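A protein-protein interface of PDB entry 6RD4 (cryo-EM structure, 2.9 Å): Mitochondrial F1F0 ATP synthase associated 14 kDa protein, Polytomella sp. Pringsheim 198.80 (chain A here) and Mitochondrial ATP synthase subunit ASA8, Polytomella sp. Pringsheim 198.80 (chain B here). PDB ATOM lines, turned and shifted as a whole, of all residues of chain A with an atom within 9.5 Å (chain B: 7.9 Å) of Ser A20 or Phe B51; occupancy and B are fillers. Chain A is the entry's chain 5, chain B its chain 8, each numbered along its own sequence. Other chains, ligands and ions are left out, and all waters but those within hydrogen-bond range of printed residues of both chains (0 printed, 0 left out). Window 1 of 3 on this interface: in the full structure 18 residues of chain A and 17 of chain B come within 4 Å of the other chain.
Among the printed residues, pairs that only touch across the chains: Ser A20 with Phe B51 (3.5 Å), Ala A19 with Phe B51 (3.6 Å), Trp A24 with Tyr B35 (3.6 Å), Thr A28 with Tyr B35 (3.6 Å), Leu A23 with Tyr B35 (3.7 Å), Trp A24 with Phe B32 (3.7 Å), Ala A16 with Phe B51 (3.7 Å), Ala A16 with Ile B55 (3.8 Å), Leu A23 with Leu B47 (3.8 Å), Ala A13 with Ile B55 (3.9 Å) and Leu A23 with His B44 (3.9 Å).
Of the printed residues of chain B, Ala A16 touches Phe B51 and Ile B55. Ser A20 touches just one residue of chain B: Phe B51. Of the printed residues of chain B, Trp A24 touches Phe B32 (3.7 Å) and Tyr B35 (3.6 Å). Of the printed residues of chain A, Phe B32 touches Trp A24. Of the printed residues of chain A, His B44 touches Leu A23 and Asp A27. Trp B45 touches none of the printed residues of chain A. No residue of chain A comes within 4 Å of Gly B49. No residue of chain A comes within 4 Å of Gly B50. Of chain A, only Ala A16 (3.7 Å), Ala A19 (3.6 Å) and Ser A20 (3.5 Å) come within 4 Å of Phe B51. Thr B52 touches none of the printed residues of chain A. Leu B57 touches none of the printed residues of chain A. The nearest residue of chain A that does not touch Phe B51 is Ala A15 (4.6 Å).
The backbone carbonyl oxygen of Ile B55 lies within hydrogen-bond range of the side-chain amide nitrogen of Gln A9 (2.7 Å). The side-chain carboxylate (OD2) of Asp A27 sits at hydrogen-bond distance from the side-chain hydroxyl (OH) of Tyr B35 (2.6 Å). OD2 of Asp A27 is in hydrogen-bond range of NE2 of His B44 (2.4 Å).
Of the 17 printed residues of chain B, 6 touch a printed residue of chain A. Hydrophobic or aromatic side chains of chain B within 4 Å of the printed part of chain A: Phe B32, Tyr B35, His B44, Leu B47, Phe B51 and Ile B55. Of the 19 printed residues of chain A, 9 touch a printed residue of chain B. Hydrophobic or aromatic side chains of chain A that line the printed part of chain B: Ala A16, Ala A19, Leu A23 and Trp A24. Among the printed residues, 14 pairs touch across the chains. Among the printed residues, no Asp or Glu carboxylate lies within 4 Å of a Lys or Arg side-chain nitrogen of the other chain.
OG of Ser A20 sits at hydrogen-bond distance from O of Ala A16 (2.7 Å). The side-chain hydroxyl of Thr A28 sits close to the backbone carbonyl oxygen of Trp A24, at 3.4 Å. O of Tyr B35 lies within hydrogen-bond range of N of Leu B40 (2.7 Å).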
ATOM      1  N   GLN A   9      15.284  22.264 -14.209  1.00  0.00           N
ATOM      2  CA  GLN A   9      16.025  22.950 -15.252  1.00  0.00           C
ATOM      3  C   GLN A   9      16.910  24.032 -14.675  1.00  0.00           C
ATOM      4  O   GLN A   9      17.943  24.352 -15.252  1.00  0.00           O
ATOM      5  CB  GLN A   9      15.064  23.557 -16.252  1.00  0.00           C
ATOM      6  CG  GLN A   9      15.676  23.983 -17.528  1.00  0.00           C
ATOM      7  CD  GLN A   9      14.658  24.521 -18.461  1.00  0.00           C
ATOM      8  OE1 GLN A   9      13.829  25.320 -18.075  1.00  0.00           O
ATOM      9  NE2 GLN A   9      14.695  24.076 -19.696  1.00  0.00           N
ATOM     10  N   GLU A  11      18.443  23.789 -11.747  1.00  0.00           N
ATOM     11  CA  GLU A  11      19.607  23.104 -11.214  1.00  0.00           C
ATOM     12  C   GLU A  11      20.452  22.457 -12.285  1.00  0.00           C
ATOM     13  O   GLU A  11      21.655  22.311 -12.098  1.00  0.00           O
ATOM     14  CB  GLU A  11      19.204  22.045 -10.210  1.00  0.00           C
ATOM     15  CG  GLU A  11      18.938  22.548  -8.840  1.00  0.00           C
ATOM     16  CD  GLU A  11      18.833  21.408  -7.855  1.00  0.00           C
ATOM     17  OE1 GLU A  11      18.751  20.257  -8.304  1.00  0.00           O
ATOM     18  OE2 GLU A  11      18.872  21.645  -6.634  1.00  0.00           O
ATOM     19  N   ALA A  12      19.859  22.019 -13.380  1.00  0.00           N
ATOM     20  CA  ALA A  12      20.664  21.495 -14.466  1.00  0.00           C
ATOM     21  C   ALA A  12      21.415  22.597 -15.171  1.00  0.00           C
ATOM     22  O   ALA A  12      22.524  22.368 -15.646  1.00  0.00           O
ATOM     23  CB  ALA A  12      19.795  20.755 -15.468  1.00  0.00           C
ATOM     24  N   ALA A  13      20.841  23.791 -15.246  1.00  0.00           N
ATOM     25  CA  ALA A  13      21.532  24.906 -15.863  1.00  0.00           C
ATOM     26  C   ALA A  13      22.553  25.520 -14.942  1.00  0.00           C
ATOM     27  O   ALA A  13      23.470  26.171 -15.420  1.00  0.00           O
ATOM     28  CB  ALA A  13      20.547  25.975 -16.291  1.00  0.00           C
ATOM     29  N   THR A  14      22.402  25.374 -13.632  1.00  0.00           N
ATOM     30  CA  THR A  14      23.472  25.776 -12.735  1.00  0.00           C
ATOM     31  C   THR A  14      24.668  24.854 -12.885  1.00  0.00           C
ATOM     32  O   THR A  14      25.809  25.298 -12.800  1.00  0.00           O
ATOM     33  CB  THR A  14      22.969  25.801 -11.301  1.00  0.00           C
ATOM     34  OG1 THR A  14      21.844  26.671 -11.215  1.00  0.00           O
ATOM     35  CG2 THR A  14      24.003  26.305 -10.370  1.00  0.00           C
ATOM     36  N   ALA A  15      24.433  23.578 -13.167  1.00  0.00           N
ATOM     37  CA  ALA A  15      25.536  22.659 -13.408  1.00  0.00           C
ATOM     38  C   ALA A  15      26.211  22.931 -14.731  1.00  0.00           C
ATOM     39  O   ALA A  15      27.412  22.727 -14.856  1.00  0.00           O
ATOM     40  CB  ALA A  15      25.045  21.222 -13.387  1.00  0.00           C
ATOM     41  N   ALA A  16      25.471  23.390 -15.721  1.00  0.00           N
ATOM     42  CA  ALA A  16      26.065  23.669 -17.013  1.00  0.00           C
ATOM     43  C   ALA A  16      26.768  25.003 -17.026  1.00  0.00           C
ATOM     44  O   ALA A  16      27.661  25.210 -17.831  1.00  0.00           O
ATOM     45  CB  ALA A  16      25.003  23.629 -18.094  1.00  0.00           C
ATOM     46  N   VAL A  17      26.370  25.926 -16.163  1.00  0.00           N
ATOM     47  CA  VAL A  17      27.069  27.196 -16.060  1.00  0.00           C
ATOM     48  C   VAL A  17      28.345  27.026 -15.265  1.00  0.00           C
ATOM     49  O   VAL A  17      29.384  27.578 -15.621  1.00  0.00           O
ATOM     50  CB  VAL A  17      26.127  28.252 -15.457  1.00  0.00           C
ATOM     51  CG1 VAL A  17      26.862  29.437 -14.943  1.00  0.00           C
ATOM     52  CG2 VAL A  17      25.179  28.706 -16.498  1.00  0.00           C
ATOM     53  N   VAL A  18      28.311  26.220 -14.212  1.00  0.00           N
ATOM     54  CA  VAL A  18      29.509  25.986 -13.422  1.00  0.00           C
ATOM     55  C   VAL A  18      30.515  25.160 -14.206  1.00  0.00           C
ATOM     56  O   VAL A  18      31.695  25.490 -14.253  1.00  0.00           O
ATOM     57  CB  VAL A  18      29.145  25.337 -12.081  1.00  0.00           C
ATOM     58  CG1 VAL A  18      30.347  24.865 -11.393  1.00  0.00           C
ATOM     59  CG2 VAL A  18      28.485  26.333 -11.213  1.00  0.00           C
ATOM     60  N   ALA A  19      30.068  24.113 -14.882  1.00  0.00           N
ATOM     61  CA  ALA A  19      31.019  23.280 -15.599  1.00  0.00           C
ATOM     62  C   ALA A  19      31.481  23.886 -16.912  1.00  0.00           C
ATOM     63  O   ALA A  19      32.490  23.441 -17.446  1.00  0.00           O
ATOM     64  CB  ALA A  19      30.436  21.905 -15.845  1.00  0.00           C
ATOM     65  N   SER A  20      30.782  24.868 -17.460  1.00  0.00           N
ATOM     66  CA  SER A  20      31.306  25.570 -18.621  1.00  0.00           C
ATOM     67  C   SER A  20      32.175  26.734 -18.234  1.00  0.00           C
ATOM     68  O   SER A  20      32.962  27.199 -19.048  1.00  0.00           O
ATOM     69  CB  SER A  20      30.194  26.107 -19.497  1.00  0.00           C
ATOM     70  OG  SER A  20      29.361  25.058 -19.903  1.00  0.00           O
ATOM     71  N   TRP A  21      32.032  27.244 -17.029  1.00  0.00           N
ATOM     72  CA  TRP A  21      33.009  28.203 -16.564  1.00  0.00           C
ATOM     73  C   TRP A  21      34.311  27.516 -16.238  1.00  0.00           C
ATOM     74  O   TRP A  21      35.378  28.070 -16.482  1.00  0.00           O
ATOM     75  CB  TRP A  21      32.496  28.947 -15.353  1.00  0.00           C
ATOM     76  CG  TRP A  21      33.405  29.995 -14.909  1.00  0.00           C
ATOM     77  CD1 TRP A  21      33.421  31.272 -15.320  1.00  0.00           C
ATOM     78  CD2 TRP A  21      34.444  29.870 -13.947  1.00  0.00           C
ATOM     79  NE1 TRP A  21      34.402  31.953 -14.686  1.00  0.00           N
ATOM     80  CE2 TRP A  21      35.046  31.105 -13.833  1.00  0.00           C
ATOM     81  CE3 TRP A  21      34.921  28.822 -13.169  1.00  0.00           C
ATOM     82  CZ2 TRP A  21      36.087  31.329 -12.988  1.00  0.00           C
ATOM     83  CZ3 TRP A  21      35.950  29.048 -12.339  1.00  0.00           C
ATOM     84  CH2 TRP A  21      36.522  30.287 -12.247  1.00  0.00           C
ATOM     85  N   VAL A  22      34.255  26.326 -15.653  1.00  0.00           N
ATOM     86  CA  VAL A  22      35.472  25.582 -15.378  1.00  0.00           C
ATOM     87  C   VAL A  22      36.118  25.135 -16.675  1.00  0.00           C
ATOM     88  O   VAL A  22      37.336  25.087 -16.782  1.00  0.00           O
ATOM     89  CB  VAL A  22      35.167  24.413 -14.431  1.00  0.00           C
ATOM     90  CG1 VAL A  22      36.359  23.594 -14.171  1.00  0.00           C
ATOM     91  CG2 VAL A  22      34.692  24.947 -13.145  1.00  0.00           C
ATOM     92  N   LEU A  23      35.327  24.877 -17.703  1.00  0.00           N
ATOM     93  CA  LEU A  23      35.908  24.570 -18.998  1.00  0.00           C
ATOM     94  C   LEU A  23      36.568  25.782 -19.608  1.00  0.00           C
ATOM     95  O   LEU A  23      37.668  25.679 -20.141  1.00  0.00           O
ATOM     96  CB  LEU A  23      34.854  24.043 -19.944  1.00  0.00           C
ATOM     97  CG  LEU A  23      35.372  23.659 -21.302  1.00  0.00           C
ATOM     98  CD1 LEU A  23      36.220  22.478 -21.134  1.00  0.00           C
ATOM     99  CD2 LEU A  23      34.210  23.345 -22.133  1.00  0.00           C
ATOM    100  N   TRP A  24      35.922  26.936 -19.532  1.00  0.00           N
ATOM    101  CA  TRP A  24      36.533  28.156 -20.028  1.00  0.00           C
ATOM    102  C   TRP A  24      37.758  28.515 -19.222  1.00  0.00           C
ATOM    103  O   TRP A  24      38.789  28.839 -19.788  1.00  0.00           O
ATOM    104  CB  TRP A  24      35.539  29.308 -20.006  1.00  0.00           C
ATOM    105  CG  TRP A  24      36.192  30.606 -20.221  1.00  0.00           C
ATOM    106  CD1 TRP A  24      36.524  31.155 -21.395  1.00  0.00           C
ATOM    107  CD2 TRP A  24      36.607  31.527 -19.221  1.00  0.00           C
ATOM    108  NE1 TRP A  24      37.132  32.352 -21.203  1.00  0.00           N
ATOM    109  CE2 TRP A  24      37.200  32.595 -19.864  1.00  0.00           C
ATOM    110  CE3 TRP A  24      36.557  31.530 -17.835  1.00  0.00           C
ATOM    111  CZ2 TRP A  24      37.720  33.655 -19.178  1.00  0.00           C
ATOM    112  CZ3 TRP A  24      37.073  32.575 -17.168  1.00  0.00           C
ATOM    113  CH2 TRP A  24      37.646  33.620 -17.830  1.00  0.00           C
ATOM    114  N   HIS A  25      37.677  28.445 -17.902  1.00  0.00           N
ATOM    115  CA  HIS A  25      38.800  28.852 -17.076  1.00  0.00           C
ATOM    116  C   HIS A  25      39.985  27.937 -17.224  1.00  0.00           C
ATOM    117  O   HIS A  25      41.116  28.397 -17.189  1.00  0.00           O
ATOM    118  CB  HIS A  25      38.400  28.891 -15.630  1.00  0.00           C
ATOM    119  CG  HIS A  25      39.324  29.697 -14.802  1.00  0.00           C
ATOM    120  ND1 HIS A  25      40.307  29.139 -14.029  1.00  0.00           N
ATOM    121  CD2 HIS A  25      39.450  31.030 -14.668  1.00  0.00           C
ATOM    122  CE1 HIS A  25      40.983  30.097 -13.430  1.00  0.00           C
ATOM    123  NE2 HIS A  25      40.485  31.254 -13.807  1.00  0.00           N
ATOM    124  N   LEU A  26      39.753  26.658 -17.423  1.00  0.00           N
ATOM    125  CA  LEU A  26      40.849  25.744 -17.653  1.00  0.00           C
ATOM    126  C   LEU A  26      41.487  25.987 -19.007  1.00  0.00           C
ATOM    127  O   LEU A  26      42.701  26.103 -19.106  1.00  0.00           O
ATOM    128  CB  LEU A  26      40.335  24.332 -17.554  1.00  0.00           C
ATOM    129  CG  LEU A  26      41.255  23.165 -17.625  1.00  0.00           C
ATOM    130  CD1 LEU A  26      41.891  23.014 -16.306  1.00  0.00           C
ATOM    131  CD2 LEU A  26      40.367  22.045 -17.929  1.00  0.00           C
ATOM    132  N   ASP A  27      40.682  26.092 -20.057  1.00  0.00           N
ATOM    133  CA  ASP A  27      41.206  26.211 -21.408  1.00  0.00           C
ATOM    134  C   ASP A  27      41.887  27.524 -21.669  1.00  0.00           C
ATOM    135  O   ASP A  27      42.755  27.604 -22.532  1.00  0.00           O
ATOM    136  CB  ASP A  27      40.098  26.113 -22.413  1.00  0.00           C
ATOM    137  CG  ASP A  27      39.895  24.760 -22.921  1.00  0.00           C
ATOM    138  OD1 ASP A  27      40.848  23.971 -22.939  1.00  0.00           O
ATOM    139  OD2 ASP A  27      38.783  24.502 -23.385  1.00  0.00           O
ATOM    140  N   THR A  28      41.463  28.569 -20.997  1.00  0.00           N
ATOM    141  CA  THR A  28      41.902  29.916 -21.281  1.00  0.00           C
ATOM    142  C   THR A  28      42.928  30.404 -20.279  1.00  0.00           C
ATOM    143  O   THR A  28      43.939  30.971 -20.659  1.00  0.00           O
ATOM    144  CB  THR A  28      40.681  30.819 -21.311  1.00  0.00           C
ATOM    145  OG1 THR A  28      39.961  30.594 -22.511  1.00  0.00           O
ATOM    146  CG2 THR A  28      41.020  32.217 -21.226  1.00  0.00           C
ATOM    147  N   PHE B  32      37.501  36.469 -25.889  1.00  0.00           N
ATOM    148  CA  PHE B  32      36.620  35.314 -25.894  1.00  0.00           C
ATOM    149  C   PHE B  32      36.253  34.892 -27.298  1.00  0.00           C
ATOM    150  O   PHE B  32      35.928  33.730 -27.503  1.00  0.00           O
ATOM    151  CB  PHE B  32      35.351  35.611 -25.099  1.00  0.00           C
ATOM    152  CG  PHE B  32      34.467  34.417 -24.887  1.00  0.00           C
ATOM    153  CD1 PHE B  32      34.727  33.523 -23.888  1.00  0.00           C
ATOM    154  CD2 PHE B  32      33.372  34.196 -25.686  1.00  0.00           C
ATOM    155  CE1 PHE B  32      33.923  32.433 -23.698  1.00  0.00           C
ATOM    156  CE2 PHE B  32      32.580  33.101 -25.498  1.00  0.00           C
ATOM    157  CZ  PHE B  32      32.861  32.225 -24.502  1.00  0.00           C
ATOM    158  N   TYR B  35      38.807  32.378 -28.376  1.00  0.00           N
ATOM    159  CA  TYR B  35      38.578  31.119 -27.699  1.00  0.00           C
ATOM    160  C   TYR B  35      37.373  30.419 -28.269  1.00  0.00           C
ATOM    161  O   TYR B  35      37.414  29.211 -28.500  1.00  0.00           O
ATOM    162  CB  TYR B  35      38.378  31.337 -26.212  1.00  0.00           C
ATOM    163  CG  TYR B  35      38.027  30.065 -25.504  1.00  0.00           C
ATOM    164  CD1 TYR B  35      38.842  28.972 -25.603  1.00  0.00           C
ATOM    165  CD2 TYR B  35      36.887  29.957 -24.752  1.00  0.00           C
ATOM    166  CE1 TYR B  35      38.538  27.838 -25.010  1.00  0.00           C
ATOM    167  CE2 TYR B  35      36.587  28.798 -24.130  1.00  0.00           C
ATOM    168  CZ  TYR B  35      37.424  27.749 -24.261  1.00  0.00           C
ATOM    169  OH  TYR B  35      37.150  26.563 -23.667  1.00  0.00           O
ATOM    170  N   LEU B  40      36.499  26.618 -28.462  1.00  0.00           N
ATOM    171  CA  LEU B  40      35.279  26.212 -27.785  1.00  0.00           C
ATOM    172  C   LEU B  40      34.302  25.557 -28.738  1.00  0.00           C
ATOM    173  O   LEU B  40      33.695  24.542 -28.408  1.00  0.00           O
ATOM    174  CB  LEU B  40      34.643  27.409 -27.108  1.00  0.00           C
ATOM    175  CG  LEU B  40      33.293  27.269 -26.458  1.00  0.00           C
ATOM    176  CD1 LEU B  40      33.368  26.275 -25.357  1.00  0.00           C
ATOM    177  CD2 LEU B  40      32.903  28.594 -25.923  1.00  0.00           C
ATOM    178  N   HIS B  44      34.975  21.711 -28.302  1.00  0.00           N
ATOM    179  CA  HIS B  44      34.101  21.418 -27.183  1.00  0.00           C
ATOM    180  C   HIS B  44      32.637  21.577 -27.524  1.00  0.00           C
ATOM    181  O   HIS B  44      31.846  21.810 -26.624  1.00  0.00           O
ATOM    182  CB  HIS B  44      34.397  22.321 -25.989  1.00  0.00           C
ATOM    183  CG  HIS B  44      35.834  22.379 -25.594  1.00  0.00           C
ATOM    184  ND1 HIS B  44      36.618  21.264 -25.445  1.00  0.00           N
ATOM    185  CD2 HIS B  44      36.616  23.430 -25.284  1.00  0.00           C
ATOM    186  CE1 HIS B  44      37.832  21.627 -25.092  1.00  0.00           C
ATOM    187  NE2 HIS B  44      37.856  22.938 -24.985  1.00  0.00           N
ATOM    188  N   TRP B  45      32.246  21.480 -28.785  1.00  0.00           N
ATOM    189  CA  TRP B  45      30.825  21.582 -29.075  1.00  0.00           C
ATOM    190  C   TRP B  45      30.066  20.326 -28.700  1.00  0.00           C
ATOM    191  O   TRP B  45      28.840  20.361 -28.631  1.00  0.00           O
ATOM    192  CB  TRP B  45      30.588  21.903 -30.544  1.00  0.00           C
ATOM    193  CG  TRP B  45      30.835  20.795 -31.482  1.00  0.00           C
ATOM    194  CD1 TRP B  45      31.994  20.494 -32.084  1.00  0.00           C
ATOM    195  CD2 TRP B  45      29.882  19.846 -31.951  1.00  0.00           C
ATOM    196  NE1 TRP B  45      31.842  19.410 -32.891  1.00  0.00           N
ATOM    197  CE2 TRP B  45      30.548  18.986 -32.813  1.00  0.00           C
ATOM    198  CE3 TRP B  45      28.531  19.628 -31.701  1.00  0.00           C
ATOM    199  CZ2 TRP B  45      29.915  17.940 -33.435  1.00  0.00           C
ATOM    200  CZ3 TRP B  45      27.919  18.597 -32.309  1.00  0.00           C
ATOM    201  CH2 TRP B  45      28.602  17.763 -33.165  1.00  0.00           C
ATOM    202  N   TYR B  46      30.761  19.222 -28.463  1.00  0.00           N
ATOM    203  CA  TYR B  46      30.115  18.038 -27.936  1.00  0.00           C
ATOM    204  C   TYR B  46      29.678  18.251 -26.500  1.00  0.00           C
ATOM    205  O   TYR B  46      28.625  17.761 -26.102  1.00  0.00           O
ATOM    206  CB  TYR B  46      31.056  16.856 -28.013  1.00  0.00           C
ATOM    207  CG  TYR B  46      31.804  16.728 -29.295  1.00  0.00           C
ATOM    208  CD1 TYR B  46      31.265  16.050 -30.356  1.00  0.00           C
ATOM    209  CD2 TYR B  46      33.065  17.250 -29.430  1.00  0.00           C
ATOM    210  CE1 TYR B  46      31.951  15.913 -31.512  1.00  0.00           C
ATOM    211  CE2 TYR B  46      33.749  17.130 -30.581  1.00  0.00           C
ATOM    212  CZ  TYR B  46      33.189  16.463 -31.619  1.00  0.00           C
ATOM    213  OH  TYR B  46      33.895  16.342 -32.783  1.00  0.00           O
ATOM    214  N   LEU B  47      30.472  18.957 -25.697  1.00  0.00           N
ATOM    215  CA  LEU B  47      30.040  19.272 -24.340  1.00  0.00           C
ATOM    216  C   LEU B  47      28.920  20.280 -24.330  1.00  0.00           C
ATOM    217  O   LEU B  47      27.994  20.162 -23.531  1.00  0.00           O
ATOM    218  CB  LEU B  47      31.163  19.835 -23.498  1.00  0.00           C
ATOM    219  CG  LEU B  47      31.949  18.960 -22.571  1.00  0.00           C
ATOM    220  CD1 LEU B  47      32.676  19.877 -21.670  1.00  0.00           C
ATOM    221  CD2 LEU B  47      31.020  18.109 -21.785  1.00  0.00           C
ATOM    222  N   LEU B  48      29.013  21.307 -25.159  1.00  0.00           N
ATOM    223  CA  LEU B  48      27.971  22.316 -25.184  1.00  0.00           C
ATOM    224  C   LEU B  48      26.687  21.764 -25.758  1.00  0.00           C
ATOM    225  O   LEU B  48      25.610  22.250 -25.433  1.00  0.00           O
ATOM    226  CB  LEU B  48      28.421  23.511 -25.998  1.00  0.00           C
ATOM    227  CG  LEU B  48      29.708  24.209 -25.613  1.00  0.00           C
ATOM    228  CD1 LEU B  48      29.784  25.450 -26.439  1.00  0.00           C
ATOM    229  CD2 LEU B  48      29.742  24.523 -24.151  1.00  0.00           C
ATOM    230  N   GLY B  49      26.779  20.762 -26.622  1.00  0.00           N
ATOM    231  CA  GLY B  49      25.592  20.053 -27.034  1.00  0.00           C
ATOM    232  C   GLY B  49      25.055  19.154 -25.954  1.00  0.00           C
ATOM    233  O   GLY B  49      23.850  18.941 -25.875  1.00  0.00           O
ATOM    234  N   GLY B  50      25.925  18.607 -25.118  1.00  0.00           N
ATOM    235  CA  GLY B  50      25.464  17.766 -24.036  1.00  0.00           C
ATOM    236  C   GLY B  50      24.881  18.545 -22.883  1.00  0.00           C
ATOM    237  O   GLY B  50      23.999  18.052 -22.189  1.00  0.00           O
ATOM    238  N   PHE B  51      25.383  19.752 -22.636  1.00  0.00           N
ATOM    239  CA  PHE B  51      24.749  20.622 -21.658  1.00  0.00           C
ATOM    240  C   PHE B  51      23.442  21.176 -22.186  1.00  0.00           C
ATOM    241  O   PHE B  51      22.547  21.480 -21.407  1.00  0.00           O
ATOM    242  CB  PHE B  51      25.672  21.775 -21.284  1.00  0.00           C
ATOM    243  CG  PHE B  51      26.834  21.383 -20.438  1.00  0.00           C
ATOM    244  CD1 PHE B  51      26.676  20.514 -19.394  1.00  0.00           C
ATOM    245  CD2 PHE B  51      28.078  21.913 -20.670  1.00  0.00           C
ATOM    246  CE1 PHE B  51      27.732  20.147 -18.616  1.00  0.00           C
ATOM    247  CE2 PHE B  51      29.135  21.560 -19.887  1.00  0.00           C
ATOM    248  CZ  PHE B  51      28.957  20.668 -18.864  1.00  0.00           C
ATOM    249  N   THR B  52      23.321  21.333 -23.500  1.00  0.00           N
ATOM    250  CA  THR B  52      22.076  21.812 -24.088  1.00  0.00           C
ATOM    251  C   THR B  52      21.013  20.733 -24.058  1.00  0.00           C
ATOM    252  O   THR B  52      19.833  21.026 -23.852  1.00  0.00           O
ATOM    253  CB  THR B  52      22.330  22.279 -25.515  1.00  0.00           C
ATOM    254  OG1 THR B  52      23.297  23.326 -25.486  1.00  0.00           O
ATOM    255  CG2 THR B  52      21.098  22.827 -26.159  1.00  0.00           C
ATOM    256  N   PHE B  53      21.409  19.477 -24.240  1.00  0.00           N
ATOM    257  CA  PHE B  53      20.454  18.384 -24.177  1.00  0.00           C
ATOM    258  C   PHE B  53      19.872  18.228 -22.785  1.00  0.00           C
ATOM    259  O   PHE B  53      18.688  17.942 -22.637  1.00  0.00           O
ATOM    260  CB  PHE B  53      21.112  17.088 -24.610  1.00  0.00           C
ATOM    261  CG  PHE B  53      20.222  15.902 -24.494  1.00  0.00           C
ATOM    262  CD1 PHE B  53      19.230  15.690 -25.413  1.00  0.00           C
ATOM    263  CD2 PHE B  53      20.383  14.992 -23.474  1.00  0.00           C
ATOM    264  CE1 PHE B  53      18.417  14.609 -25.313  1.00  0.00           C
ATOM    265  CE2 PHE B  53      19.564  13.917 -23.371  1.00  0.00           C
ATOM    266  CZ  PHE B  53      18.586  13.724 -24.292  1.00  0.00           C
ATOM    267  N   THR B  54      20.679  18.420 -21.755  1.00  0.00           N
ATOM    268  CA  THR B  54      20.196  18.234 -20.399  1.00  0.00           C
ATOM    269  C   THR B  54      19.271  19.353 -19.968  1.00  0.00           C
ATOM    270  O   THR B  54      18.267  19.095 -19.310  1.00  0.00           O
ATOM    271  CB  THR B  54      21.378  18.137 -19.463  1.00  0.00           C
ATOM    272  OG1 THR B  54      22.208  17.074 -19.904  1.00  0.00           O
ATOM    273  CG2 THR B  54      20.949  17.834 -18.087  1.00  0.00           C
ATOM    274  N   ILE B  55      19.570  20.589 -20.343  1.00  0.00           N
ATOM    275  CA  ILE B  55      18.713  21.708 -19.978  1.00  0.00           C
ATOM    276  C   ILE B  55      17.391  21.626 -20.723  1.00  0.00           C
ATOM    277  O   ILE B  55      16.335  21.970 -20.189  1.00  0.00           O
ATOM    278  CB  ILE B  55      19.468  23.020 -20.241  1.00  0.00           C
ATOM    279  CG1 ILE B  55      20.652  23.116 -19.312  1.00  0.00           C
ATOM    280  CG2 ILE B  55      18.610  24.216 -20.028  1.00  0.00           C
ATOM    281  CD1 ILE B  55      21.604  24.167 -19.699  1.00  0.00           C
ATOM    282  N   THR B  56      17.418  21.117 -21.948  1.00  0.00           N
ATOM    283  CA  THR B  56      16.193  20.863 -22.686  1.00  0.00           C
ATOM    284  C   THR B  56      15.410  19.695 -22.118  1.00  0.00           C
ATOM    285  O   THR B  56      14.197  19.809 -21.949  1.00  0.00           O
ATOM    286  CB  THR B  56      16.525  20.590 -24.139  1.00  0.00           C
ATOM    287  OG1 THR B  56      17.276  21.686 -24.651  1.00  0.00           O
ATOM    288  CG2 THR B  56      15.285  20.457 -24.943  1.00  0.00           C
ATOM    289  N   LEU B  57      16.075  18.590 -21.791  1.00  0.00           N
ATOM    290  CA  LEU B  57      15.383  17.419 -21.268  1.00  0.00           C
ATOM    291  C   LEU B  57      14.805  17.687 -19.898  1.00  0.00           C
ATOM    292  O   LEU B  57      13.718  17.214 -19.577  1.00  0.00           O
ATOM    293  CB  LEU B  57      16.336  16.235 -21.203  1.00  0.00           C
ATOM    294  CG  LEU B  57      15.904  14.988 -20.453  1.00  0.00           C
ATOM    295  CD1 LEU B  57      14.945  14.219 -21.294  1.00  0.00           C
ATOM    296  CD2 LEU B  57      17.082  14.150 -20.086  1.00  0.00           C
